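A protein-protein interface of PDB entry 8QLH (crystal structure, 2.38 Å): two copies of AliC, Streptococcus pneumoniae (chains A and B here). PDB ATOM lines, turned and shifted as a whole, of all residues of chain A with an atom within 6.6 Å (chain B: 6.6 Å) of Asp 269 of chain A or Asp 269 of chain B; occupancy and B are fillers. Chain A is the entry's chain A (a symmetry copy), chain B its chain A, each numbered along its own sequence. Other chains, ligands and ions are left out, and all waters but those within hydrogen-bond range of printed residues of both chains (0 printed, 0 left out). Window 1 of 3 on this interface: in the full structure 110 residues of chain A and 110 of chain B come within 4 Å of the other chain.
The backbone NH of Lys 270 of chain B lies within hydrogen-bond range of the backbone carbonyl oxygen of Tyr 267 of chain A (2.9 Å).
The backbone carbonyl oxygen (O) of Tyr 267 of chain B sits close to the side-chain carboxylate (OD1) of Asp 269 of chain A.
The backbone carbonyl oxygen (O) of Tyr 267 of chain A sits close to the side-chain carboxylate (OD1) of Asp 269 of chain B (3.2 Å).
O of Tyr 267 of chain B lies within hydrogen-bond range of N of Lys 270 of chain A.
O of Ile 271 of chain B is in hydrogen-bond range of OG1 of Thr 603 of chain B (2.6 Å).
The backbone NH of Lys 270 of chain A sits close to the side-chain hydroxyl of Thr 603 of chain A (3.4 Å).
The backbone NH of Lys 270 of chain B sits close to the side-chain hydroxyl of Thr 603 of chain B (3.4 Å).
The backbone NH of Ile 271 of chain A lies within hydrogen-bond range of the side-chain carboxylate of Asp 269 of chain A (3.2 Å).
The backbone carbonyl oxygen of Ile 271 of chain A lies within hydrogen-bond range of the side-chain hydroxyl of Thr 603 of chain A, 2.6 Å away.
The backbone carbonyl oxygen (O) of Asp 269 of chain A sits at hydrogen-bond distance from the backbone NH (N) of Thr 603 of chain A, 2.9 Å away.
Among the printed residues, merely in contact across the chains: Asp 269 of chain A with Asp 269 of chain B (3.5 Å), Gly 268 of chain A with Asp 269 of chain B (3.5 Å), Asp 269 of chain A with Gly 268 of chain B (3.5 Å), Lys 264 of chain A with Ile 271 of chain B (3.9 Å), Ile 271 of chain A with Lys 264 of chain B (3.9 Å), Tyr 267 of chain A with Ile 271 of chain B (3.9 Å) and Ile 271 of chain A with Tyr 267 of chain B (3.9 Å).
Of chain B, only Tyr 267 (3.2 Å), Gly 268 (3.5 Å) and Asp 269 (3.5 Å) come within 4 Å of Asp 269 of chain A.
Asp 269 of chain B touches three residues of chain A.
Of the printed residues of chain A, Lys 270 of chain B touches Tyr 267.
Of the printed residues of chain B, Tyr 267 of chain A touches Asp 269 (3.2 Å), Lys 270 (2.9 Å) and Ile 271 (3.9 Å).
Of the printed residues of chain B, Lys 264 of chain A touches Ile 271 (3.9 Å).
Val 272 of chain B touches none of the printed residues of chain A.
The nearest residue of chain B that does not touch Asp 269 of chain A is Lys 264 of chain B (5.3 Å).
The nearest residue of chain A that does not touch Asp 269 of chain B is Lys 264 of chain A (5.3 Å).
Of the 13 printed residues of chain A, 6 touch a printed residue of chain B.
Hydrophobic or aromatic side chains of chain A within 4 Å of the printed part of chain B: Ile 271.
Hydrophobic or aromatic side chains of chain B that line the printed part of chain A: Ile 271.
Among the printed residues, no Asp or Glu carboxylate lies within 4 Å of a Lys or Arg side-chain nitrogen of the other chain.
Tyr 267 of chain A touches Lys 270 of chain B, and with the chains exchanged Lys 270 of chain A touches Tyr 267 of chain B.
Tyr 267 of chain A touches Ile 271 of chain B, and with the chains exchanged Ile 271 of chain A touches Tyr 267 of chain B.
Gly 268 of chain A touches Asp 269 of chain B, and with the chains exchanged Asp 269 of chain A touches Gly 268 of chain B.
Asp 269 of chain A touches its own counterpart, Asp 269 of chain B.
Positions printed for both chains: 264, 265, 267, 268, 269, 270, 271, 272, 601, 602, 603, 604 and 605.
Of the 11 pairs that touch across the chains among the printed residues, 11 have their exchanged pair printed and touching as well.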
ATOM      1  N   LYS A 264     -30.404  11.069  13.966  1.00  0.00           N
ATOM      2  CA  LYS A 264     -29.030  11.364  14.454  1.00  0.00           C
ATOM      3  C   LYS A 264     -29.072  12.346  15.631  1.00  0.00           C
ATOM      4  O   LYS A 264     -28.309  12.128  16.594  1.00  0.00           O
ATOM      5  CB  LYS A 264     -28.168  11.914  13.313  1.00  0.00           C
ATOM      6  CG  LYS A 264     -27.821  10.913  12.219  1.00  0.00           C
ATOM      7  CD  LYS A 264     -27.093  11.536  11.046  1.00  0.00           C
ATOM      8  CE  LYS A 264     -25.725  12.071  11.417  1.00  0.00           C
ATOM      9  NZ  LYS A 264     -24.989  12.566  10.229  1.00  0.00           N
ATOM     10  N   LYS A 265     -29.920  13.379  15.568  1.00  0.00           N
ATOM     11  CA  LYS A 265     -29.946  14.345  16.660  1.00  0.00           C
ATOM     12  C   LYS A 265     -30.746  13.828  17.854  1.00  0.00           C
ATOM     13  O   LYS A 265     -30.459  14.207  18.995  1.00  0.00           O
ATOM     14  CB  LYS A 265     -30.473  15.697  16.176  1.00  0.00           C
ATOM     15  CG  LYS A 265     -31.808  15.650  15.501  1.00  0.00           C
ATOM     16  CD  LYS A 265     -32.279  17.045  15.150  1.00  0.00           C
ATOM     17  CE  LYS A 265     -32.688  17.812  16.392  1.00  0.00           C
ATOM     18  NZ  LYS A 265     -33.548  16.997  17.299  1.00  0.00           N
ATOM     19  N   TYR A 267     -30.611  10.684  18.909  1.00  0.00           N
ATOM     20  CA  TYR A 267     -29.737   9.729  19.578  1.00  0.00           C
ATOM     21  C   TYR A 267     -28.276  10.165  19.568  1.00  0.00           C
ATOM     22  O   TYR A 267     -27.385   9.342  19.805  1.00  0.00           O
ATOM     23  CB  TYR A 267     -29.881   8.345  18.942  1.00  0.00           C
ATOM     24  CG  TYR A 267     -31.178   7.660  19.293  1.00  0.00           C
ATOM     25  CD1 TYR A 267     -31.306   6.927  20.470  1.00  0.00           C
ATOM     26  CD2 TYR A 267     -32.281   7.754  18.455  1.00  0.00           C
ATOM     27  CE1 TYR A 267     -32.504   6.305  20.799  1.00  0.00           C
ATOM     28  CE2 TYR A 267     -33.480   7.137  18.776  1.00  0.00           C
ATOM     29  CZ  TYR A 267     -33.587   6.415  19.947  1.00  0.00           C
ATOM     30  OH  TYR A 267     -34.787   5.808  20.260  1.00  0.00           O
ATOM     31  N   GLY A 268     -28.012  11.443  19.305  1.00  0.00           N
ATOM     32  CA  GLY A 268     -26.663  11.960  19.289  1.00  0.00           C
ATOM     33  C   GLY A 268     -26.317  12.704  20.567  1.00  0.00           C
ATOM     34  O   GLY A 268     -27.164  12.958  21.421  1.00  0.00           O
ATOM     35  N   ASP A 269     -25.033  13.045  20.677  1.00  0.00           N
ATOM     36  CA  ASP A 269     -24.530  13.736  21.856  1.00  0.00           C
ATOM     37  C   ASP A 269     -25.202  15.097  22.001  1.00  0.00           C
ATOM     38  O   ASP A 269     -25.390  15.822  21.022  1.00  0.00           O
ATOM     39  CB  ASP A 269     -23.009  13.897  21.758  1.00  0.00           C
ATOM     40  CG  ASP A 269     -22.382  14.390  23.052  1.00  0.00           C
ATOM     41  OD1 ASP A 269     -23.064  14.357  24.097  1.00  0.00           O
ATOM     42  OD2 ASP A 269     -21.201  14.804  23.025  1.00  0.00           O
ATOM     43  N   LYS A 270     -25.571  15.438  23.234  1.00  0.00           N
ATOM     44  CA  LYS A 270     -26.250  16.693  23.508  1.00  0.00           C
ATOM     45  C   LYS A 270     -25.545  17.547  24.554  1.00  0.00           C
ATOM     46  O   LYS A 270     -26.037  18.634  24.869  1.00  0.00           O
ATOM     47  CB  LYS A 270     -27.700  16.430  23.953  1.00  0.00           C
ATOM     48  CG  LYS A 270     -28.599  15.948  22.822  1.00  0.00           C
ATOM     49  CD  LYS A 270     -29.898  15.385  23.350  1.00  0.00           C
ATOM     50  CE  LYS A 270     -30.471  14.345  22.401  1.00  0.00           C
ATOM     51  NZ  LYS A 270     -31.018  14.989  21.179  1.00  0.00           N
ATOM     52  N   ILE A 271     -24.421  17.098  25.097  1.00  0.00           N
ATOM     53  CA  ILE A 271     -23.690  17.873  26.092  1.00  0.00           C
ATOM     54  C   ILE A 271     -22.753  18.837  25.380  1.00  0.00           C
ATOM     55  O   ILE A 271     -22.005  18.446  24.476  1.00  0.00           O
ATOM     56  CB  ILE A 271     -22.927  16.954  27.058  1.00  0.00           C
ATOM     57  CG1 ILE A 271     -23.927  16.166  27.909  1.00  0.00           C
ATOM     58  CG2 ILE A 271     -22.001  17.762  27.953  1.00  0.00           C
ATOM     59  CD1 ILE A 271     -23.286  15.311  28.985  1.00  0.00           C
ATOM     60  N   VAL A 272     -22.814  20.107  25.767  1.00  0.00           N
ATOM     61  CA  VAL A 272     -21.986  21.143  25.169  1.00  0.00           C
ATOM     62  C   VAL A 272     -21.290  21.902  26.288  1.00  0.00           C
ATOM     63  O   VAL A 272     -21.792  21.996  27.413  1.00  0.00           O
ATOM     64  CB  VAL A 272     -22.794  22.111  24.267  1.00  0.00           C
ATOM     65  CG1 VAL A 272     -23.788  21.345  23.402  1.00  0.00           C
ATOM     66  CG2 VAL A 272     -23.522  23.144  25.090  1.00  0.00           C
ATOM     67  N   VAL A 601     -30.708  21.044  22.109  1.00  0.00           N
ATOM     68  CA  VAL A 601     -29.624  21.391  21.199  1.00  0.00           C
ATOM     69  C   VAL A 601     -28.537  20.328  21.279  1.00  0.00           C
ATOM     70  O   VAL A 601     -28.006  20.037  22.357  1.00  0.00           O
ATOM     71  CB  VAL A 601     -29.067  22.780  21.537  1.00  0.00           C
ATOM     72  CG1 VAL A 601     -27.804  23.044  20.745  1.00  0.00           C
ATOM     73  CG2 VAL A 601     -30.111  23.842  21.251  1.00  0.00           C
ATOM     74  N   THR A 602     -28.196  19.745  20.134  1.00  0.00           N
ATOM     75  CA  THR A 602     -27.162  18.725  20.100  1.00  0.00           C
ATOM     76  C   THR A 602     -25.775  19.364  20.057  1.00  0.00           C
ATOM     77  O   THR A 602     -25.608  20.528  19.687  1.00  0.00           O
ATOM     78  CB  THR A 602     -27.359  17.805  18.895  1.00  0.00           C
ATOM     79  OG1 THR A 602     -26.846  18.437  17.716  1.00  0.00           O
ATOM     80  CG2 THR A 602     -28.835  17.529  18.695  1.00  0.00           C
ATOM     81  N   THR A 603     -24.772  18.571  20.448  1.00  0.00           N
ATOM     82  CA  THR A 603     -23.395  19.059  20.503  1.00  0.00           C
ATOM     83  C   THR A 603     -22.894  19.485  19.129  1.00  0.00           C
ATOM     84  O   THR A 603     -22.159  20.472  19.009  1.00  0.00           O
ATOM     85  CB  THR A 603     -22.485  17.976  21.086  1.00  0.00           C
ATOM     86  OG1 THR A 603     -23.031  17.517  22.328  1.00  0.00           O
ATOM     87  CG2 THR A 603     -21.085  18.521  21.328  1.00  0.00           C
ATOM     88  N   LYS A 604     -23.270  18.749  18.081  1.00  0.00           N
ATOM     89  CA  LYS A 604     -22.844  19.114  16.735  1.00  0.00           C
ATOM     90  C   LYS A 604     -23.481  20.424  16.286  1.00  0.00           C
ATOM     91  O   LYS A 604     -22.808  21.274  15.694  1.00  0.00           O
ATOM     92  CB  LYS A 604     -23.172  17.987  15.758  1.00  0.00           C
ATOM     93  CG  LYS A 604     -22.044  16.972  15.600  1.00  0.00           C
ATOM     94  CD  LYS A 604     -22.492  15.762  14.791  1.00  0.00           C
ATOM     95  CE  LYS A 604     -21.310  14.881  14.408  1.00  0.00           C
ATOM     96  NZ  LYS A 604     -20.672  14.234  15.589  1.00  0.00           N
ATOM     97  N   GLU A 605     -24.775  20.606  16.562  1.00  0.00           N
ATOM     98  CA  GLU A 605     -25.442  21.853  16.200  1.00  0.00           C
ATOM     99  C   GLU A 605     -24.880  23.026  16.988  1.00  0.00           C
ATOM    100  O   GLU A 605     -24.742  24.132  16.453  1.00  0.00           O
ATOM    101  CB  GLU A 605     -26.948  21.741  16.433  1.00  0.00           C
ATOM    102  CG  GLU A 605     -27.659  20.748  15.539  1.00  0.00           C
ATOM    103  CD  GLU A 605     -29.129  20.611  15.884  1.00  0.00           C
ATOM    104  OE1 GLU A 605     -29.486  20.849  17.057  1.00  0.00           O
ATOM    105  OE2 GLU A 605     -29.923  20.260  14.984  1.00  0.00           O
ATOM    106  N   LYS B 264     -23.574  11.588  31.435  1.00  0.00           N
ATOM    107  CA  LYS B 264     -22.869  11.608  30.125  1.00  0.00           C
ATOM    108  C   LYS B 264     -23.436  10.534  29.189  1.00  0.00           C
ATOM    109  O   LYS B 264     -23.606  10.842  27.992  1.00  0.00           O
ATOM    110  CB  LYS B 264     -21.363  11.417  30.329  1.00  0.00           C
ATOM    111  CG  LYS B 264     -20.644  12.579  31.003  1.00  0.00           C
ATOM    112  CD  LYS B 264     -19.191  12.286  31.312  1.00  0.00           C
ATOM    113  CE  LYS B 264     -18.350  12.085  30.068  1.00  0.00           C
ATOM    114  NZ  LYS B 264     -16.915  11.919  30.397  1.00  0.00           N
ATOM    115  N   LYS B 265     -23.718   9.330  29.699  1.00  0.00           N
ATOM    116  CA  LYS B 265     -24.221   8.284  28.816  1.00  0.00           C
ATOM    117  C   LYS B 265     -25.711   8.454  28.528  1.00  0.00           C
ATOM    118  O   LYS B 265     -26.179   8.048  27.459  1.00  0.00           O
ATOM    119  CB  LYS B 265     -23.916   6.899  29.389  1.00  0.00           C
ATOM    120  CG  LYS B 265     -24.404   6.669  30.784  1.00  0.00           C
ATOM    121  CD  LYS B 265     -24.139   5.244  31.217  1.00  0.00           C
ATOM    122  CE  LYS B 265     -25.060   4.275  30.500  1.00  0.00           C
ATOM    123  NZ  LYS B 265     -26.476   4.746  30.494  1.00  0.00           N
ATOM    124  N   TYR B 267     -27.131  11.404  27.982  1.00  0.00           N
ATOM    125  CA  TYR B 267     -27.217  12.479  27.001  1.00  0.00           C
ATOM    126  C   TYR B 267     -26.082  12.435  25.984  1.00  0.00           C
ATOM    127  O   TYR B 267     -25.832  13.431  25.296  1.00  0.00           O
ATOM    128  CB  TYR B 267     -27.246  13.836  27.706  1.00  0.00           C
ATOM    129  CG  TYR B 267     -28.560  14.126  28.387  1.00  0.00           C
ATOM    130  CD1 TYR B 267     -29.626  14.678  27.683  1.00  0.00           C
ATOM    131  CD2 TYR B 267     -28.741  13.838  29.732  1.00  0.00           C
ATOM    132  CE1 TYR B 267     -30.840  14.935  28.307  1.00  0.00           C
ATOM    133  CE2 TYR B 267     -29.949  14.091  30.364  1.00  0.00           C
ATOM    134  CZ  TYR B 267     -30.994  14.638  29.648  1.00  0.00           C
ATOM    135  OH  TYR B 267     -32.195  14.882  30.285  1.00  0.00           O
ATOM    136  N   GLY B 268     -25.394  11.301  25.870  1.00  0.00           N
ATOM    137  CA  GLY B 268     -24.312  11.152  24.924  1.00  0.00           C
ATOM    138  C   GLY B 268     -24.737  10.396  23.678  1.00  0.00           C
ATOM    139  O   GLY B 268     -25.834   9.848  23.593  1.00  0.00           O
ATOM    140  N   ASP B 269     -23.830  10.387  22.702  1.00  0.00           N
ATOM    141  CA  ASP B 269     -24.094   9.732  21.428  1.00  0.00           C
ATOM    142  C   ASP B 269     -24.309   8.237  21.634  1.00  0.00           C
ATOM    143  O   ASP B 269     -23.597   7.591  22.406  1.00  0.00           O
ATOM    144  CB  ASP B 269     -22.928   9.978  20.464  1.00  0.00           C
ATOM    145  CG  ASP B 269     -23.233   9.533  19.042  1.00  0.00           C
ATOM    146  OD1 ASP B 269     -24.417   9.284  18.735  1.00  0.00           O
ATOM    147  OD2 ASP B 269     -22.287   9.442  18.228  1.00  0.00           O
ATOM    148  N   LYS B 270     -25.305   7.689  20.941  1.00  0.00           N
ATOM    149  CA  LYS B 270     -25.640   6.281  21.067  1.00  0.00           C
ATOM    150  C   LYS B 270     -25.631   5.535  19.740  1.00  0.00           C
ATOM    151  O   LYS B 270     -25.906   4.331  19.728  1.00  0.00           O
ATOM    152  CB  LYS B 270     -27.015   6.117  21.740  1.00  0.00           C
ATOM    153  CG  LYS B 270     -27.005   6.464  23.222  1.00  0.00           C
ATOM    154  CD  LYS B 270     -28.408   6.618  23.764  1.00  0.00           C
ATOM    155  CE  LYS B 270     -28.437   7.567  24.950  1.00  0.00           C
ATOM    156  NZ  LYS B 270     -27.833   6.932  26.150  1.00  0.00           N
ATOM    157  N   ILE B 271     -25.329   6.200  18.632  1.00  0.00           N
ATOM    158  CA  ILE B 271     -25.288   5.542  17.332  1.00  0.00           C
ATOM    159  C   ILE B 271     -23.911   4.928  17.129  1.00  0.00           C
ATOM    160  O   ILE B 271     -22.884   5.587  17.331  1.00  0.00           O
ATOM    161  CB  ILE B 271     -25.642   6.522  16.204  1.00  0.00           C
ATOM    162  CG1 ILE B 271     -27.110   6.937  16.330  1.00  0.00           C
ATOM    163  CG2 ILE B 271     -25.389   5.893  14.844  1.00  0.00           C
ATOM    164  CD1 ILE B 271     -27.605   7.814  15.196  1.00  0.00           C
ATOM    165  N   VAL B 272     -23.887   3.652  16.757  1.00  0.00           N
ATOM    166  CA  VAL B 272     -22.644   2.929  16.535  1.00  0.00           C
ATOM    167  C   VAL B 272     -22.715   2.264  15.170  1.00  0.00           C
ATOM    168  O   VAL B 272     -23.795   1.931  14.670  1.00  0.00           O
ATOM    169  CB  VAL B 272     -22.353   1.883  17.642  1.00  0.00           C
ATOM    170  CG1 VAL B 272     -22.661   2.452  19.022  1.00  0.00           C
ATOM    171  CG2 VAL B 272     -23.147   0.620  17.420  1.00  0.00           C
ATOM    172  N   VAL B 601     -26.686   1.097  24.644  1.00  0.00           N
ATOM    173  CA  VAL B 601     -25.233   1.133  24.550  1.00  0.00           C
ATOM    174  C   VAL B 601     -24.802   2.427  23.870  1.00  0.00           C
ATOM    175  O   VAL B 601     -25.231   2.732  22.751  1.00  0.00           O
ATOM    176  CB  VAL B 601     -24.716  -0.093  23.787  1.00  0.00           C
ATOM    177  CG1 VAL B 601     -23.237   0.058  23.495  1.00  0.00           C
ATOM    178  CG2 VAL B 601     -24.977  -1.352  24.590  1.00  0.00           C
ATOM    179  N   THR B 602     -23.948   3.190  24.542  1.00  0.00           N
ATOM    180  CA  THR B 602     -23.466   4.439  23.977  1.00  0.00           C
ATOM    181  C   THR B 602     -22.309   4.186  23.013  1.00  0.00           C
ATOM    182  O   THR B 602     -21.646   3.147  23.055  1.00  0.00           O
ATOM    183  CB  THR B 602     -23.031   5.395  25.088  1.00  0.00           C
ATOM    184  OG1 THR B 602     -21.721   5.039  25.545  1.00  0.00           O
ATOM    185  CG2 THR B 602     -23.995   5.302  26.253  1.00  0.00           C
ATOM    186  N   THR B 603     -22.077   5.165  22.134  1.00  0.00           N
ATOM    187  CA  THR B 603     -21.030   5.045  21.121  1.00  0.00           C
ATOM    188  C   THR B 603     -19.651   4.903  21.751  1.00  0.00           C
ATOM    189  O   THR B 603     -18.805   4.155  21.246  1.00  0.00           O
ATOM    190  CB  THR B 603     -21.065   6.260  20.192  1.00  0.00           C
ATOM    191  OG1 THR B 603     -22.396   6.434  19.692  1.00  0.00           O
ATOM    192  CG2 THR B 603     -20.114   6.071  19.019  1.00  0.00           C
ATOM    193  N   LYS B 604     -19.398   5.620  22.848  1.00  0.00           N
ATOM    194  CA  LYS B 604     -18.104   5.516  23.514  1.00  0.00           C
ATOM    195  C   LYS B 604     -17.911   4.139  24.138  1.00  0.00           C
ATOM    196  O   LYS B 604     -16.827   3.554  24.035  1.00  0.00           O
ATOM    197  CB  LYS B 604     -17.967   6.614  24.566  1.00  0.00           C
ATOM    198  CG  LYS B 604     -17.337   7.895  24.028  1.00  0.00           C
ATOM    199  CD  LYS B 604     -17.416   9.025  25.046  1.00  0.00           C
ATOM    200  CE  LYS B 604     -16.563  10.214  24.624  1.00  0.00           C
ATOM    201  NZ  LYS B 604     -17.077  10.880  23.394  1.00  0.00           N
ATOM    202  N   GLU B 605     -18.950   3.603  24.784  1.00  0.00           N
ATOM    203  CA  GLU B 605     -18.851   2.270  25.371  1.00  0.00           C
ATOM    204  C   GLU B 605     -18.687   1.207  24.296  1.00  0.00           C
ATOM    205  O   GLU B 605     -17.948   0.233  24.485  1.00  0.00           O
ATOM    206  CB  GLU B 605     -20.085   1.968  26.222  1.00  0.00           C
ATOM    207  CG  GLU B 605     -20.234   2.830  27.456  1.00  0.00           C
ATOM    208  CD  GLU B 605     -21.523   2.550  28.203  1.00  0.00           C
ATOM    209  OE1 GLU B 605     -22.497   2.110  27.556  1.00  0.00           O
ATOM    210  OE2 GLU B 605     -21.563   2.774  29.432  1.00  0.00           O
